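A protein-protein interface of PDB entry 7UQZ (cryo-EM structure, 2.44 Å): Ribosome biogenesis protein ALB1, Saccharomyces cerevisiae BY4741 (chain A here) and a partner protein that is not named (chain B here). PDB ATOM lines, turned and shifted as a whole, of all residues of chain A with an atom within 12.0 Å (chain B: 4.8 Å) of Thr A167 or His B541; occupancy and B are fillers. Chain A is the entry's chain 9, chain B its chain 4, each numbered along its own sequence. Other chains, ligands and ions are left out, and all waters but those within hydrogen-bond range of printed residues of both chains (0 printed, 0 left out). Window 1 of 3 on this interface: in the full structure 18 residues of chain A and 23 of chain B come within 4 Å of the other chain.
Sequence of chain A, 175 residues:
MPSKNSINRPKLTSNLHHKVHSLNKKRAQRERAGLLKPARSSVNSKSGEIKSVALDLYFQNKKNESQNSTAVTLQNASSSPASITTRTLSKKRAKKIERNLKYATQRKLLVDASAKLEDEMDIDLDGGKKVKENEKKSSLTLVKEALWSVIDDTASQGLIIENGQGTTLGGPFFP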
ATOM      1  N   GLN A 165      24.881 -17.466  12.658  1.00  0.00           N
ATOM      2  CA  GLN A 165      24.251 -16.625  13.668  1.00  0.00           C
ATOM      3  C   GLN A 165      25.150 -16.475  14.889  1.00  0.00           C
ATOM      4  O   GLN A 165      25.982 -15.571  14.953  1.00  0.00           O
ATOM      5  CB  GLN A 165      22.896 -17.206  14.079  1.00  0.00           C
ATOM      6  CG  GLN A 165      21.909 -17.347  12.933  1.00  0.00           C
ATOM      7  CD  GLN A 165      21.436 -16.009  12.399  1.00  0.00           C
ATOM      8  OE1 GLN A 165      21.357 -15.026  13.135  1.00  0.00           O
ATOM      9  NE2 GLN A 165      21.120 -15.967  11.110  1.00  0.00           N
ATOM     10  N   GLY A 166      24.976 -17.367  15.860  1.00  0.00           N
ATOM     11  CA  GLY A 166      25.793 -17.341  17.056  1.00  0.00           C
ATOM     12  C   GLY A 166      25.017 -16.974  18.302  1.00  0.00           C
ATOM     13  O   GLY A 166      23.990 -17.585  18.606  1.00  0.00           O
ATOM     14  N   THR A 167      25.504 -15.974  19.034  1.00  0.00           N
ATOM     15  CA  THR A 167      24.858 -15.539  20.262  1.00  0.00           C
ATOM     16  C   THR A 167      25.064 -14.042  20.428  1.00  0.00           C
ATOM     17  O   THR A 167      25.994 -13.455  19.871  1.00  0.00           O
ATOM     18  CB  THR A 167      25.403 -16.286  21.483  1.00  0.00           C
ATOM     19  OG1 THR A 167      24.726 -15.838  22.664  1.00  0.00           O
ATOM     20  CG2 THR A 167      26.884 -16.020  21.634  1.00  0.00           C
ATOM     21  N   THR A 168      24.174 -13.427  21.204  1.00  0.00           N
ATOM     22  CA  THR A 168      24.248 -11.997  21.469  1.00  0.00           C
ATOM     23  C   THR A 168      23.644 -11.722  22.837  1.00  0.00           C
ATOM     24  O   THR A 168      22.493 -12.088  23.094  1.00  0.00           O
ATOM     25  CB  THR A 168      23.516 -11.189  20.392  1.00  0.00           C
ATOM     26  OG1 THR A 168      24.141 -11.403  19.120  1.00  0.00           O
ATOM     27  CG2 THR A 168      23.553  -9.706  20.721  1.00  0.00           C
ATOM     28  N   LEU A 169      24.421 -11.083  23.704  1.00  0.00           N
ATOM     29  CA  LEU A 169      23.977 -10.716  25.039  1.00  0.00           C
ATOM     30  C   LEU A 169      24.039  -9.204  25.200  1.00  0.00           C
ATOM     31  O   LEU A 169      24.800  -8.516  24.515  1.00  0.00           O
ATOM     32  CB  LEU A 169      24.830 -11.394  26.121  1.00  0.00           C
ATOM     33  CG  LEU A 169      24.887 -12.923  26.107  1.00  0.00           C
ATOM     34  CD1 LEU A 169      25.665 -13.435  27.308  1.00  0.00           C
ATOM     35  CD2 LEU A 169      23.491 -13.526  26.071  1.00  0.00           C
ATOM     36  N   GLY A 170      23.221  -8.692  26.115  1.00  0.00           N
ATOM     37  CA  GLY A 170      23.190  -7.269  26.369  1.00  0.00           C
ATOM     38  C   GLY A 170      22.475  -6.495  25.272  1.00  0.00           C
ATOM     39  O   GLY A 170      21.765  -7.043  24.430  1.00  0.00           O
ATOM     40  N   GLY A 171      22.686  -5.181  25.301  1.00  0.00           N
ATOM     41  CA  GLY A 171      22.070  -4.290  24.349  1.00  0.00           C
ATOM     42  C   GLY A 171      22.787  -2.959  24.262  1.00  0.00           C
ATOM     43  O   GLY A 171      23.771  -2.709  24.966  1.00  0.00           O
ATOM     44  N   ASP B 182      33.549 -14.053  23.266  1.00  0.00           N
ATOM     45  CA  ASP B 182      33.401 -15.492  23.471  1.00  0.00           C
ATOM     46  C   ASP B 182      33.538 -15.853  24.944  1.00  0.00           C
ATOM     47  O   ASP B 182      32.740 -16.628  25.485  1.00  0.00           O
ATOM     48  CB  ASP B 182      34.441 -16.255  22.645  1.00  0.00           C
ATOM     49  CG  ASP B 182      34.398 -15.905  21.172  1.00  0.00           C
ATOM     50  OD1 ASP B 182      33.301 -15.628  20.651  1.00  0.00           O
ATOM     51  OD2 ASP B 182      35.470 -15.908  20.529  1.00  0.00           O
ATOM     52  N   ALA B 185      30.460 -14.545  26.991  1.00  0.00           N
ATOM     53  CA  ALA B 185      29.285 -15.373  26.736  1.00  0.00           C
ATOM     54  C   ALA B 185      29.409 -16.737  27.402  1.00  0.00           C
ATOM     55  O   ALA B 185      28.447 -17.230  28.005  1.00  0.00           O
ATOM     56  CB  ALA B 185      29.070 -15.530  25.232  1.00  0.00           C
ATOM     57  N   SER B 233      32.256 -25.442  23.396  1.00  0.00           N
ATOM     58  CA  SER B 233      31.390 -24.853  22.382  1.00  0.00           C
ATOM     59  C   SER B 233      31.813 -23.427  22.059  1.00  0.00           C
ATOM     60  O   SER B 233      31.769 -23.010  20.896  1.00  0.00           O
ATOM     61  CB  SER B 233      29.937 -24.883  22.852  1.00  0.00           C
ATOM     62  OG  SER B 233      29.540 -26.198  23.199  1.00  0.00           O
ATOM     63  N   TYR B 234      32.223 -22.665  23.071  1.00  0.00           N
ATOM     64  CA  TYR B 234      32.618 -21.280  22.863  1.00  0.00           C
ATOM     65  C   TYR B 234      34.118 -21.103  22.666  1.00  0.00           C
ATOM     66  O   TYR B 234      34.591 -19.961  22.633  1.00  0.00           O
ATOM     67  CB  TYR B 234      32.125 -20.414  24.020  1.00  0.00           C
ATOM     68  CG  TYR B 234      30.695 -19.991  23.822  1.00  0.00           C
ATOM     69  CD1 TYR B 234      29.649 -20.818  24.203  1.00  0.00           C
ATOM     70  CD2 TYR B 234      30.389 -18.781  23.219  1.00  0.00           C
ATOM     71  CE1 TYR B 234      28.339 -20.442  24.006  1.00  0.00           C
ATOM     72  CE2 TYR B 234      29.085 -18.398  23.020  1.00  0.00           C
ATOM     73  CZ  TYR B 234      28.063 -19.230  23.415  1.00  0.00           C
ATOM     74  OH  TYR B 234      26.758 -18.850  23.215  1.00  0.00           O
ATOM     75  N   ASN B 235      34.867 -22.201  22.530  1.00  0.00           N
ATOM     76  CA  ASN B 235      36.308 -22.169  22.253  1.00  0.00           C
ATOM     77  C   ASN B 235      37.057 -21.427  23.360  1.00  0.00           C
ATOM     78  O   ASN B 235      37.861 -20.526  23.113  1.00  0.00           O
ATOM     79  CB  ASN B 235      36.600 -21.561  20.876  1.00  0.00           C
ATOM     80  CG  ASN B 235      38.013 -21.848  20.394  1.00  0.00           C
ATOM     81  OD1 ASN B 235      38.637 -22.824  20.809  1.00  0.00           O
ATOM     82  ND2 ASN B 235      38.521 -20.993  19.516  1.00  0.00           N
ATOM     83  N   ILE B 537      27.689  -7.840  23.841  1.00  0.00           N
ATOM     84  CA  ILE B 537      28.700  -8.631  23.155  1.00  0.00           C
ATOM     85  C   ILE B 537      28.040  -9.369  22.000  1.00  0.00           C
ATOM     86  O   ILE B 537      26.822  -9.554  21.961  1.00  0.00           O
ATOM     87  CB  ILE B 537      29.404  -9.640  24.088  1.00  0.00           C
ATOM     88  CG1 ILE B 537      28.405 -10.689  24.577  1.00  0.00           C
ATOM     89  CG2 ILE B 537      30.062  -8.931  25.261  1.00  0.00           C
ATOM     90  CD1 ILE B 537      29.041 -11.848  25.288  1.00  0.00           C
ATOM     91  N   HIS B 538      28.867  -9.786  21.046  1.00  0.00           N
ATOM     92  CA  HIS B 538      28.423 -10.637  19.951  1.00  0.00           C
ATOM     93  C   HIS B 538      29.508 -11.657  19.648  1.00  0.00           C
ATOM     94  O   HIS B 538      30.672 -11.292  19.461  1.00  0.00           O
ATOM     95  CB  HIS B 538      28.104  -9.823  18.693  1.00  0.00           C
ATOM     96  CG  HIS B 538      27.730 -10.665  17.515  1.00  0.00           C
ATOM     97  ND1 HIS B 538      26.460 -11.166  17.331  1.00  0.00           N
ATOM     98  CD2 HIS B 538      28.463 -11.106  16.466  1.00  0.00           C
ATOM     99  CE1 HIS B 538      26.425 -11.874  16.217  1.00  0.00           C
ATOM    100  NE2 HIS B 538      27.627 -11.854  15.672  1.00  0.00           N
ATOM    101  N   SER B 539      29.122 -12.926  19.592  1.00  0.00           N
ATOM    102  CA  SER B 539      30.052 -14.015  19.345  1.00  0.00           C
ATOM    103  C   SER B 539      29.591 -14.828  18.146  1.00  0.00           C
ATOM    104  O   SER B 539      28.391 -14.984  17.905  1.00  0.00           O
ATOM    105  CB  SER B 539      30.184 -14.924  20.571  1.00  0.00           C
ATOM    106  OG  SER B 539      31.046 -16.016  20.307  1.00  0.00           O
ATOM    107  N   GLN B 540      30.560 -15.349  17.399  1.00  0.00           N
ATOM    108  CA  GLN B 540      30.289 -16.195  16.246  1.00  0.00           C
ATOM    109  C   GLN B 540      30.070 -17.654  16.625  1.00  0.00           C
ATOM    110  O   GLN B 540      29.806 -18.475  15.741  1.00  0.00           O
ATOM    111  CB  GLN B 540      31.438 -16.096  15.237  1.00  0.00           C
ATOM    112  CG  GLN B 540      31.720 -14.686  14.752  1.00  0.00           C
ATOM    113  CD  GLN B 540      32.916 -14.620  13.823  1.00  0.00           C
ATOM    114  OE1 GLN B 540      33.637 -15.603  13.650  1.00  0.00           O
ATOM    115  NE2 GLN B 540      33.132 -13.458  13.218  1.00  0.00           N
ATOM    116  N   HIS B 541      30.177 -17.993  17.905  1.00  0.00           N
ATOM    117  CA  HIS B 541      29.974 -19.351  18.383  1.00  0.00           C
ATOM    118  C   HIS B 541      28.653 -19.449  19.132  1.00  0.00           C
ATOM    119  O   HIS B 541      28.126 -18.459  19.645  1.00  0.00           O
ATOM    120  CB  HIS B 541      31.124 -19.792  19.295  1.00  0.00           C
ATOM    121  CG  HIS B 541      32.479 -19.627  18.684  1.00  0.00           C
ATOM    122  ND1 HIS B 541      32.904 -20.367  17.602  1.00  0.00           N
ATOM    123  CD2 HIS B 541      33.509 -18.812  19.009  1.00  0.00           C
ATOM    124  CE1 HIS B 541      34.136 -20.011  17.283  1.00  0.00           C
ATOM    125  NE2 HIS B 541      34.526 -19.068  18.122  1.00  0.00           N
ATOM    126  N   GLU B 542      28.122 -20.668  19.191  1.00  0.00           N
ATOM    127  CA  GLU B 542      26.877 -20.928  19.897  1.00  0.00           C
ATOM    128  C   GLU B 542      26.831 -22.398  20.280  1.00  0.00           C
ATOM    129  O   GLU B 542      27.586 -23.219  19.752  1.00  0.00           O
ATOM    130  CB  GLU B 542      25.657 -20.555  19.048  1.00  0.00           C
ATOM    131  CG  GLU B 542      25.535 -21.352  17.759  1.00  0.00           C
ATOM    132  CD  GLU B 542      24.246 -21.064  17.016  1.00  0.00           C
ATOM    133  OE1 GLU B 542      23.396 -20.332  17.564  1.00  0.00           O
ATOM    134  OE2 GLU B 542      24.084 -21.569  15.886  1.00  0.00           O
ATOM    135  N   LEU B 543      25.941 -22.715  21.215  1.00  0.00           N
ATOM    136  CA  LEU B 543      25.721 -24.102  21.598  1.00  0.00           C
ATOM    137  C   LEU B 543      25.102 -24.876  20.440  1.00  0.00           C
ATOM    138  O   LEU B 543      24.249 -24.361  19.712  1.00  0.00           O
ATOM    139  CB  LEU B 543      24.818 -24.174  22.829  1.00  0.00           C
ATOM    140  CG  LEU B 543      25.366 -23.554  24.117  1.00  0.00           C
ATOM    141  CD1 LEU B 543      24.326 -23.611  25.222  1.00  0.00           C
ATOM    142  CD2 LEU B 543      26.640 -24.257  24.547  1.00  0.00           C
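O of Gln A165 touches CE1 of His B538, 3.9 Å away.
O of Gln A165 touches O of Ser B539, at 3.9 Å.
Ser B539 touches Gly A166.
Gly A166 touches His B541.
Thr A167 touches Tyr B234 (CG2 to OH, 3.2 Å).
O of His B541 touches CG2 of Thr A167, at 3.4 Å.
Ile B537 touches Thr A168 (O to CG2, 3.5 Å).
Printed residues of chain B within 4 Å of Gly A166: Ser B539 (3.6 Å), His B541 (3.7 Å) and Glu B542 (3.0 Å).
Of chain B, only Tyr B234 (3.2 Å), His B538 (3.5 Å), Ser B539 (3.2 Å) and His B541 (3.4 Å) come within 4 Å of Thr A167.
Printed residues of chain B within 4 Å of Thr A168: Ile B537 and His B538.
Asp B182 touches none of the printed residues of chain A.
Ala B185 touches none of the printed residues of chain A.
Ser B233 touches none of the printed residues of chain A.
Of chain A, only Thr A167 (3.2 Å) comes within 4 Å of Tyr B234.
No residue of chain A comes within 4 Å of Asn B235.
Of the printed residues of chain A, Ile B537 touches Thr A168 and Leu A169.
Gln B540 touches none of the printed residues of chain A.
Of chain A, only Gly A166 comes within 4 Å of Glu B542.
The nearest residue of chain B that does not touch Thr A167 is Ala B185 (4.2 Å).
Printed residues of chain B that touch a printed residue of chain A: Tyr B234, Ile B537, His B538, Ser B539, His B541 and Glu B542.
Along chain B the printed residues that touch a printed residue of chain A span positions 234 to 542.
Hydrophobic or aromatic side chains of chain A within 4 Å of the printed part of chain B: Leu A169.
Among the printed residues, 12 pairs touch across the chains.
A ring nitrogen (ND1) of His B538 is in hydrogen-bond range of the backbone carbonyl oxygen of Thr A167, 3.5 Å away.
N of Ile B537 is in hydrogen-bond range of O of Leu A169.
The side-chain carboxylate (OE1) of Glu B542 lies close to the backbone carbonyl oxygen (O) of Gly A166 (3.0 Å).
OG1 of Thr A168 is in hydrogen-bond range of ND1 of His B538 (2.9 Å).
The backbone carbonyl oxygen (O) of Thr A167 sits at hydrogen-bond distance from the backbone NH (N) of Ser B539 (3.2 Å).
The side-chain hydroxyl of Ser B539 lies close to the backbone NH of His B541 (3.2 Å).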
